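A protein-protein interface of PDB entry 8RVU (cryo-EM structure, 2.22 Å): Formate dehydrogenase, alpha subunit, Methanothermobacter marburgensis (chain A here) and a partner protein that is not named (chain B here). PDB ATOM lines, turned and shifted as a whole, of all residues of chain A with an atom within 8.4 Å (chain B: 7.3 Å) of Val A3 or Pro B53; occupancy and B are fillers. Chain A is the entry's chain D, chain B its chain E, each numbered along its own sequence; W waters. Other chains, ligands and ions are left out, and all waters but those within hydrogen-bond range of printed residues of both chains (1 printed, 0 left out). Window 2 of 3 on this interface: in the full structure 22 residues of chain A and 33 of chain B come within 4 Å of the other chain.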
ATOM      1  N   MET A   2       6.524  -8.300   9.877  1.00  0.00           N
ATOM      2  CA  MET A   2       5.854  -7.407  10.813  1.00  0.00           C
ATOM      3  C   MET A   2       4.548  -8.026  11.302  1.00  0.00           C
ATOM      4  O   MET A   2       4.374  -8.254  12.497  1.00  0.00           O
ATOM      5  CB  MET A   2       5.585  -6.048  10.161  1.00  0.00           C
ATOM      6  CG  MET A   2       6.828  -5.172  10.017  1.00  0.00           C
ATOM      7  SD  MET A   2       7.050  -3.901  11.287  1.00  0.00           S
ATOM      8  CE  MET A   2       5.416  -3.174  11.411  1.00  0.00           C
ATOM      9  N   VAL A   3       3.640  -8.307  10.372  1.00  0.00           N
ATOM     10  CA  VAL A   3       2.351  -8.922  10.675  1.00  0.00           C
ATOM     11  C   VAL A   3       2.404 -10.366  10.199  1.00  0.00           C
ATOM     12  O   VAL A   3       2.598 -10.624   9.005  1.00  0.00           O
ATOM     13  CB  VAL A   3       1.193  -8.164  10.008  1.00  0.00           C
ATOM     14  CG1 VAL A   3      -0.144  -8.656  10.541  1.00  0.00           C
ATOM     15  CG2 VAL A   3       1.346  -6.666  10.217  1.00  0.00           C
ATOM     16  N   LYS A   4       2.230 -11.310  11.126  1.00  0.00           N
ATOM     17  CA  LYS A   4       2.352 -12.725  10.801  1.00  0.00           C
ATOM     18  C   LYS A   4       1.208 -13.522  11.414  1.00  0.00           C
ATOM     19  O   LYS A   4       0.829 -13.292  12.564  1.00  0.00           O
ATOM     20  CB  LYS A   4       3.693 -13.287  11.287  1.00  0.00           C
ATOM     21  CG  LYS A   4       4.899 -12.689  10.579  1.00  0.00           C
ATOM     22  CD  LYS A   4       6.179 -13.450  10.905  1.00  0.00           C
ATOM     23  CE  LYS A   4       7.059 -13.658   9.679  1.00  0.00           C
ATOM     24  NZ  LYS A   4       8.442 -13.154   9.903  1.00  0.00           N
ATOM     25  N   HIS A   5       0.681 -14.474  10.644  1.00  0.00           N
ATOM     26  CA  HIS A   5      -0.402 -15.329  11.115  1.00  0.00           C
ATOM     27  C   HIS A   5       0.069 -16.223  12.258  1.00  0.00           C
ATOM     28  O   HIS A   5       1.247 -16.575  12.356  1.00  0.00           O
ATOM     29  CB  HIS A   5      -0.925 -16.207   9.977  1.00  0.00           C
ATOM     30  CG  HIS A   5      -1.599 -15.446   8.879  1.00  0.00           C
ATOM     31  ND1 HIS A   5      -2.268 -14.260   9.094  1.00  0.00           N
ATOM     32  CD2 HIS A   5      -1.704 -15.703   7.554  1.00  0.00           C
ATOM     33  CE1 HIS A   5      -2.759 -13.822   7.949  1.00  0.00           C
ATOM     34  NE2 HIS A   5      -2.431 -14.679   6.999  1.00  0.00           N
ATOM     35  N   THR A   6      -0.869 -16.600  13.123  1.00  0.00           N
ATOM     36  CA  THR A   6      -0.571 -17.546  14.191  1.00  0.00           C
ATOM     37  C   THR A   6      -1.878 -17.978  14.842  1.00  0.00           C
ATOM     38  O   THR A   6      -2.954 -17.458  14.536  1.00  0.00           O
ATOM     39  CB  THR A   6       0.384 -16.944  15.229  1.00  0.00           C
ATOM     40  OG1 THR A   6       0.840 -17.970  16.119  1.00  0.00           O
ATOM     41  CG2 THR A   6      -0.309 -15.856  16.034  1.00  0.00           C
ATOM     42  N   VAL A  17      -5.027 -15.434  14.836  1.00  0.00           N
ATOM     43  CA  VAL A  17      -4.686 -14.047  15.118  1.00  0.00           C
ATOM     44  C   VAL A  17      -3.479 -13.678  14.267  1.00  0.00           C
ATOM     45  O   VAL A  17      -2.842 -14.536  13.651  1.00  0.00           O
ATOM     46  CB  VAL A  17      -4.382 -13.810  16.614  1.00  0.00           C
ATOM     47  CG1 VAL A  17      -5.571 -14.212  17.464  1.00  0.00           C
ATOM     48  CG2 VAL A  17      -3.140 -14.575  17.042  1.00  0.00           C
ATOM     49  N   ASN A  18      -3.169 -12.385  14.225  1.00  0.00           N
ATOM     50  CA  ASN A  18      -1.936 -11.904  13.624  1.00  0.00           C
ATOM     51  C   ASN A  18      -1.108 -11.227  14.701  1.00  0.00           C
ATOM     52  O   ASN A  18      -1.637 -10.442  15.489  1.00  0.00           O
ATOM     53  CB  ASN A  18      -2.227 -10.924  12.486  1.00  0.00           C
ATOM     54  CG  ASN A  18      -2.717 -11.613  11.234  1.00  0.00           C
ATOM     55  OD1 ASN A  18      -2.248 -12.692  10.884  1.00  0.00           O
ATOM     56  ND2 ASN A  18      -3.670 -10.992  10.554  1.00  0.00           N
ATOM     57  N   ILE A  19       0.182 -11.530  14.738  1.00  0.00           N
ATOM     58  CA  ILE A  19       1.112 -10.861  15.635  1.00  0.00           C
ATOM     59  C   ILE A  19       1.816  -9.765  14.854  1.00  0.00           C
ATOM     60  O   ILE A  19       2.371 -10.017  13.775  1.00  0.00           O
ATOM     61  CB  ILE A  19       2.120 -11.850  16.245  1.00  0.00           C
ATOM     62  CG1 ILE A  19       1.412 -12.763  17.248  1.00  0.00           C
ATOM     63  CG2 ILE A  19       3.259 -11.097  16.919  1.00  0.00           C
ATOM     64  CD1 ILE A  19       2.252 -13.929  17.722  1.00  0.00           C
ATOM     65  N   VAL A  20       1.755  -8.545  15.379  1.00  0.00           N
ATOM     66  CA  VAL A  20       2.475  -7.403  14.834  1.00  0.00           C
ATOM     67  C   VAL A  20       3.792  -7.313  15.592  1.00  0.00           C
ATOM     68  O   VAL A  20       3.805  -7.037  16.796  1.00  0.00           O
ATOM     69  CB  VAL A  20       1.667  -6.105  14.971  1.00  0.00           C
ATOM     70  CG1 VAL A  20       2.507  -4.903  14.553  1.00  0.00           C
ATOM     71  CG2 VAL A  20       0.389  -6.182  14.151  1.00  0.00           C
ATOM     72  N   GLU A  21       4.891  -7.543  14.880  1.00  0.00           N
ATOM     73  CA  GLU A  21       6.235  -7.556  15.439  1.00  0.00           C
ATOM     74  C   GLU A  21       7.000  -6.347  14.923  1.00  0.00           C
ATOM     75  O   GLU A  21       7.012  -6.083  13.715  1.00  0.00           O
ATOM     76  CB  GLU A  21       6.964  -8.851  15.062  1.00  0.00           C
ATOM     77  CG  GLU A  21       8.475  -8.816  15.248  1.00  0.00           C
ATOM     78  CD  GLU A  21       9.218  -8.648  13.933  1.00  0.00           C
ATOM     79  OE1 GLU A  21       9.029  -9.491  13.031  1.00  0.00           O
ATOM     80  OE2 GLU A  21       9.989  -7.674  13.801  1.00  0.00           O
ATOM     81  N   MET A  22       7.634  -5.616  15.836  1.00  0.00           N
ATOM     82  CA  MET A  22       8.430  -4.439  15.503  1.00  0.00           C
ATOM     83  C   MET A  22       9.858  -4.679  15.973  1.00  0.00           C
ATOM     84  O   MET A  22      10.116  -4.749  17.181  1.00  0.00           O
ATOM     85  CB  MET A  22       7.846  -3.183  16.147  1.00  0.00           C
ATOM     86  CG  MET A  22       6.696  -2.562  15.373  1.00  0.00           C
ATOM     87  SD  MET A  22       7.257  -1.531  14.008  1.00  0.00           S
ATOM     88  CE  MET A  22       7.661  -0.019  14.877  1.00  0.00           C
ATOM     89  N   GLY A  28       2.050  -6.054  18.987  1.00  0.00           N
ATOM     90  CA  GLY A  28       0.612  -5.923  18.917  1.00  0.00           C
ATOM     91  C   GLY A  28      -0.068  -7.114  18.283  1.00  0.00           C
ATOM     92  O   GLY A  28       0.566  -8.114  17.944  1.00  0.00           O
ATOM     93  N   THR A  29      -1.383  -6.981  18.115  1.00  0.00           N
ATOM     94  CA  THR A  29      -2.209  -7.990  17.472  1.00  0.00           C
ATOM     95  C   THR A  29      -3.004  -7.343  16.346  1.00  0.00           C
ATOM     96  O   THR A  29      -3.349  -6.160  16.408  1.00  0.00           O
ATOM     97  CB  THR A  29      -3.163  -8.655  18.484  1.00  0.00           C
ATOM     98  OG1 THR A  29      -2.462  -9.673  19.207  1.00  0.00           O
ATOM     99  CG2 THR A  29      -4.362  -9.283  17.785  1.00  0.00           C
ATOM    100  N   TYR A  30      -3.287  -8.131  15.313  1.00  0.00           N
ATOM    101  CA  TYR A  30      -4.070  -7.700  14.169  1.00  0.00           C
ATOM    102  C   TYR A  30      -5.112  -8.757  13.827  1.00  0.00           C
ATOM    103  O   TYR A  30      -4.885  -9.957  14.044  1.00  0.00           O
ATOM    104  CB  TYR A  30      -3.168  -7.440  12.950  1.00  0.00           C
ATOM    105  CG  TYR A  30      -3.727  -6.442  11.959  1.00  0.00           C
ATOM    106  CD1 TYR A  30      -3.789  -5.091  12.267  1.00  0.00           C
ATOM    107  CD2 TYR A  30      -4.187  -6.851  10.713  1.00  0.00           C
ATOM    108  CE1 TYR A  30      -4.295  -4.173  11.367  1.00  0.00           C
ATOM    109  CE2 TYR A  30      -4.696  -5.939   9.805  1.00  0.00           C
ATOM    110  CZ  TYR A  30      -4.747  -4.602  10.138  1.00  0.00           C
ATOM    111  OH  TYR A  30      -5.251  -3.688   9.241  1.00  0.00           O
ATOM    112  N   PRO A  31      -6.270  -8.344  13.301  1.00  0.00           N
ATOM    113  CA  PRO A  31      -7.329  -9.319  12.998  1.00  0.00           C
ATOM    114  C   PRO A  31      -6.924 -10.260  11.871  1.00  0.00           C
ATOM    115  O   PRO A  31      -6.423  -9.830  10.832  1.00  0.00           O
ATOM    116  CB  PRO A  31      -8.519  -8.442  12.593  1.00  0.00           C
ATOM    117  CG  PRO A  31      -8.240  -7.114  13.181  1.00  0.00           C
ATOM    118  CD  PRO A  31      -6.753  -6.961  13.140  1.00  0.00           C
ATOM    119  N   TYR A  32      -7.158 -11.552  12.090  1.00  0.00           N
ATOM    120  CA  TYR A  32      -6.922 -12.576  11.074  1.00  0.00           C
ATOM    121  C   TYR A  32      -8.258 -12.934  10.422  1.00  0.00           C
ATOM    122  O   TYR A  32      -8.861 -13.979  10.675  1.00  0.00           O
ATOM    123  CB  TYR A  32      -6.242 -13.787  11.712  1.00  0.00           C
ATOM    124  CG  TYR A  32      -5.736 -14.850  10.756  1.00  0.00           C
ATOM    125  CD1 TYR A  32      -6.003 -14.795   9.393  1.00  0.00           C
ATOM    126  CD2 TYR A  32      -4.985 -15.919  11.229  1.00  0.00           C
ATOM    127  CE1 TYR A  32      -5.537 -15.772   8.533  1.00  0.00           C
ATOM    128  CE2 TYR A  32      -4.517 -16.899  10.377  1.00  0.00           C
ATOM    129  CZ  TYR A  32      -4.795 -16.821   9.031  1.00  0.00           C
ATOM    130  OH  TYR A  32      -4.328 -17.794   8.180  1.00  0.00           O
ATOM    131  N   ARG A  33      -8.715 -12.028   9.555  1.00  0.00           N
ATOM    132  CA  ARG A  33     -10.062 -12.122   9.001  1.00  0.00           C
ATOM    133  C   ARG A  33     -10.264 -13.371   8.154  1.00  0.00           C
ATOM    134  O   ARG A  33     -11.394 -13.859   8.049  1.00  0.00           O
ATOM    135  CB  ARG A  33     -10.367 -10.881   8.159  1.00  0.00           C
ATOM    136  CG  ARG A  33     -10.840  -9.685   8.967  1.00  0.00           C
ATOM    137  CD  ARG A  33     -11.212  -8.513   8.072  1.00  0.00           C
ATOM    138  NE  ARG A  33     -11.588  -7.336   8.844  1.00  0.00           N
ATOM    139  CZ  ARG A  33     -10.732  -6.439   9.317  1.00  0.00           C
ATOM    140  NH1 ARG A  33      -9.429  -6.546   9.109  1.00  0.00           N
ATOM    141  NH2 ARG A  33     -11.193  -5.408  10.017  1.00  0.00           N
ATOM    142  N   ALA A 320       5.934 -17.268  14.001  1.00  0.00           N
ATOM    143  CA  ALA A 320       5.566 -15.863  13.874  1.00  0.00           C
ATOM    144  C   ALA A 320       6.634 -14.953  14.462  1.00  0.00           C
ATOM    145  O   ALA A 320       6.719 -13.778  14.087  1.00  0.00           O
ATOM    146  CB  ALA A 320       4.222 -15.603  14.555  1.00  0.00           C
ATOM    147  N   LEU B  40       3.755   2.330   4.045  1.00  0.00           N
ATOM    148  CA  LEU B  40       2.810   1.389   4.633  1.00  0.00           C
ATOM    149  C   LEU B  40       1.728   1.077   3.608  1.00  0.00           C
ATOM    150  O   LEU B  40       0.987   1.974   3.193  1.00  0.00           O
ATOM    151  CB  LEU B  40       2.195   1.958   5.911  1.00  0.00           C
ATOM    152  CG  LEU B  40       1.107   1.107   6.570  1.00  0.00           C
ATOM    153  CD1 LEU B  40       1.632  -0.278   6.913  1.00  0.00           C
ATOM    154  CD2 LEU B  40       0.564   1.795   7.811  1.00  0.00           C
ATOM    155  N   THR B  41       1.638  -0.187   3.199  1.00  0.00           N
ATOM    156  CA  THR B  41       0.680  -0.591   2.176  1.00  0.00           C
ATOM    157  C   THR B  41       0.174  -1.990   2.513  1.00  0.00           C
ATOM    158  O   THR B  41       0.406  -2.508   3.606  1.00  0.00           O
ATOM    159  CB  THR B  41       1.316  -0.515   0.780  1.00  0.00           C
ATOM    160  OG1 THR B  41       2.606  -1.139   0.800  1.00  0.00           O
ATOM    161  CG2 THR B  41       1.454   0.931   0.329  1.00  0.00           C
ATOM    162  N   LEU B  42      -0.544  -2.597   1.573  1.00  0.00           N
ATOM    163  CA  LEU B  42      -1.054  -3.953   1.706  1.00  0.00           C
ATOM    164  C   LEU B  42      -0.289  -4.899   0.792  1.00  0.00           C
ATOM    165  O   LEU B  42       0.302  -4.483  -0.209  1.00  0.00           O
ATOM    166  CB  LEU B  42      -2.547  -4.021   1.361  1.00  0.00           C
ATOM    167  CG  LEU B  42      -3.594  -3.735   2.442  1.00  0.00           C
ATOM    168  CD1 LEU B  42      -4.928  -4.325   2.015  1.00  0.00           C
ATOM    169  CD2 LEU B  42      -3.193  -4.283   3.803  1.00  0.00           C
ATOM    170  N   GLU B  43      -0.308  -6.182   1.148  1.00  0.00           N
ATOM    171  CA  GLU B  43       0.232  -7.237   0.302  1.00  0.00           C
ATOM    172  C   GLU B  43      -0.630  -8.477   0.480  1.00  0.00           C
ATOM    173  O   GLU B  43      -0.991  -8.824   1.607  1.00  0.00           O
ATOM    174  CB  GLU B  43       1.692  -7.543   0.653  1.00  0.00           C
ATOM    175  CG  GLU B  43       2.455  -8.265  -0.446  1.00  0.00           C
ATOM    176  CD  GLU B  43       3.582  -9.129   0.086  1.00  0.00           C
ATOM    177  OE1 GLU B  43       3.467  -9.636   1.222  1.00  0.00           O
ATOM    178  OE2 GLU B  43       4.587  -9.301  -0.634  1.00  0.00           O
ATOM    179  N   GLY B  51      -5.292 -10.287   2.910  1.00  0.00           N
ATOM    180  CA  GLY B  51      -4.494  -9.075   2.812  1.00  0.00           C
ATOM    181  C   GLY B  51      -3.779  -8.809   4.126  1.00  0.00           C
ATOM    182  O   GLY B  51      -4.364  -8.951   5.201  1.00  0.00           O
ATOM    183  N   ILE B  52      -2.511  -8.421   4.031  1.00  0.00           N
ATOM    184  CA  ILE B  52      -1.670  -8.231   5.208  1.00  0.00           C
ATOM    185  C   ILE B  52      -0.952  -6.892   5.081  1.00  0.00           C
ATOM    186  O   ILE B  52      -0.375  -6.602   4.023  1.00  0.00           O
ATOM    187  CB  ILE B  52      -0.667  -9.385   5.360  1.00  0.00           C
ATOM    188  CG1 ILE B  52      -1.346 -10.718   5.024  1.00  0.00           C
ATOM    189  CG2 ILE B  52      -0.096  -9.408   6.770  1.00  0.00           C
ATOM    190  CD1 ILE B  52      -0.591 -11.942   5.501  1.00  0.00           C
ATOM    191  N   PRO B  53      -0.972  -6.037   6.105  1.00  0.00           N
ATOM    192  CA  PRO B  53      -0.183  -4.802   6.034  1.00  0.00           C
ATOM    193  C   PRO B  53       1.307  -5.099   5.943  1.00  0.00           C
ATOM    194  O   PRO B  53       1.810  -6.047   6.549  1.00  0.00           O
ATOM    195  CB  PRO B  53      -0.538  -4.072   7.335  1.00  0.00           C
ATOM    196  CG  PRO B  53      -1.806  -4.696   7.804  1.00  0.00           C
ATOM    197  CD  PRO B  53      -1.758  -6.114   7.347  1.00  0.00           C
ATOM    198  N   VAL B  54       2.010  -4.273   5.175  1.00  0.00           N
ATOM    199  CA  VAL B  54       3.451  -4.390   4.997  1.00  0.00           C
ATOM    200  C   VAL B  54       4.064  -3.000   5.090  1.00  0.00           C
ATOM    201  O   VAL B  54       3.493  -2.018   4.599  1.00  0.00           O
ATOM    202  CB  VAL B  54       3.813  -5.057   3.652  1.00  0.00           C
ATOM    203  CG1 VAL B  54       3.487  -6.539   3.692  1.00  0.00           C
ATOM    204  CG2 VAL B  54       3.090  -4.376   2.498  1.00  0.00           C
ATOM    205  N   LEU B  55       5.228  -2.923   5.730  1.00  0.00           N
ATOM    206  CA  LEU B  55       5.999  -1.691   5.859  1.00  0.00           C
ATOM    207  C   LEU B  55       7.295  -1.865   5.078  1.00  0.00           C
ATOM    208  O   LEU B  55       8.211  -2.560   5.529  1.00  0.00           O
ATOM    209  CB  LEU B  55       6.279  -1.373   7.326  1.00  0.00           C
ATOM    210  CG  LEU B  55       6.862   0.013   7.601  1.00  0.00           C
ATOM    211  CD1 LEU B  55       5.841   1.094   7.298  1.00  0.00           C
ATOM    212  CD2 LEU B  55       7.343   0.117   9.037  1.00  0.00           C
ATOM    213  N   THR B  74      -9.232  -3.251   5.659  1.00  0.00           N
ATOM    214  CA  THR B  74      -8.193  -2.969   6.637  1.00  0.00           C
ATOM    215  C   THR B  74      -8.226  -1.505   7.060  1.00  0.00           C
ATOM    216  O   THR B  74      -8.784  -0.644   6.376  1.00  0.00           O
ATOM    217  CB  THR B  74      -6.813  -3.315   6.067  1.00  0.00           C
ATOM    218  OG1 THR B  74      -6.640  -2.672   4.798  1.00  0.00           O
ATOM    219  CG2 THR B  74      -6.671  -4.822   5.893  1.00  0.00           C
ATOM    220  N   MET B  75      -7.620  -1.237   8.216  1.00  0.00           N
ATOM    221  CA  MET B  75      -7.479   0.112   8.750  1.00  0.00           C
ATOM    222  C   MET B  75      -6.013   0.353   9.076  1.00  0.00           C
ATOM    223  O   MET B  75      -5.395  -0.448   9.784  1.00  0.00           O
ATOM    224  CB  MET B  75      -8.350   0.305  10.000  1.00  0.00           C
ATOM    225  CG  MET B  75      -8.197   1.665  10.681  1.00  0.00           C
ATOM    226  SD  MET B  75      -8.856   3.068   9.752  1.00  0.00           S
ATOM    227  CE  MET B  75     -10.438   2.439   9.196  1.00  0.00           C
ATOM    228  N   PHE B  76      -5.462   1.455   8.562  1.00  0.00           N
ATOM    229  CA  PHE B  76      -4.056   1.783   8.762  1.00  0.00           C
ATOM    230  C   PHE B  76      -3.825   2.877   9.794  1.00  0.00           C
ATOM    231  O   PHE B  76      -2.702   3.000  10.295  1.00  0.00           O
ATOM    232  CB  PHE B  76      -3.418   2.232   7.439  1.00  0.00           C
ATOM    233  CG  PHE B  76      -3.125   1.111   6.473  1.00  0.00           C
ATOM    234  CD1 PHE B  76      -2.884  -0.182   6.914  1.00  0.00           C
ATOM    235  CD2 PHE B  76      -3.078   1.362   5.111  1.00  0.00           C
ATOM    236  CE1 PHE B  76      -2.613  -1.194   6.019  1.00  0.00           C
ATOM    237  CE2 PHE B  76      -2.806   0.350   4.213  1.00  0.00           C
ATOM    238  CZ  PHE B  76      -2.575  -0.927   4.669  1.00  0.00           C
ATOM    239  N   LEU B  79      -2.636   1.648  13.191  1.00  0.00           N
ATOM    240  CA  LEU B  79      -1.281   1.122  13.057  1.00  0.00           C
ATOM    241  C   LEU B  79      -0.255   2.247  13.105  1.00  0.00           C
ATOM    242  O   LEU B  79       0.734   2.170  13.846  1.00  0.00           O
ATOM    243  CB  LEU B  79      -1.153   0.344  11.746  1.00  0.00           C
ATOM    244  CG  LEU B  79      -1.530  -1.138  11.755  1.00  0.00           C
ATOM    245  CD1 LEU B  79      -1.435  -1.706  10.350  1.00  0.00           C
ATOM    246  CD2 LEU B  79      -0.648  -1.924  12.706  1.00  0.00           C
HETATM  247  O   HOH W   1      -8.132  -3.885   9.989  1.00  0.00           O
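Hydrophobic or aromatic side chains of chain B within 4 Å of the printed part of chain A: Ile B52, Pro B53 and Leu B79.
Of the 18 printed residues of chain A, 3 touch a printed residue of chain B.
Hydrophobic or aromatic side chains of chain A that line the printed part of chain B: Val A3, His A5 and Tyr A30.
Among the printed residues, 7 pairs touch across the chains.
Val A3 touches two residues of chain B.
Pro B53 touches two residues of chain A.
No residue of chain A comes within 4 Å of Val B54.
Printed residues of chain A within 4 Å of Ile B52: Val A3 and His A5.
Of the printed residues of chain A, Met B75 touches Tyr A30 (3.3 Å).
The nearest residue of chain A that does not touch Pro B53 is Met A2 (5.2 Å).
The nearest printed residue of chain A that does not touch Thr B74 is Arg A33 (4.5 Å).
Among the printed residues, merely in contact across the chains: Tyr A30 with Thr B74, His A5 with Ile B52, Val A3 with Ile B52, Tyr A30 with Pro B53, Val A3 with Pro B53 and Tyr A30 with Leu B79.
The backbone NH (N) of His A5 sits close to the side-chain amide oxygen (OD1) of Asn A18.
O of Glu B43 is in hydrogen-bond range of N of Ile B52 (2.9 Å).
The backbone carbonyl oxygen (O) of Asn A18 sits at hydrogen-bond distance from the backbone NH (N) of Tyr A30 (2.8 Å).
Water W1 lies within hydrogen-bond range of OH of Tyr A30 (3.0 Å), NH1 of Arg A33 (3.1 Å) and N of Met B75 (3.2 Å).
O of Met B75 is in hydrogen-bond range of OH of Tyr A30 (3.3 Å).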
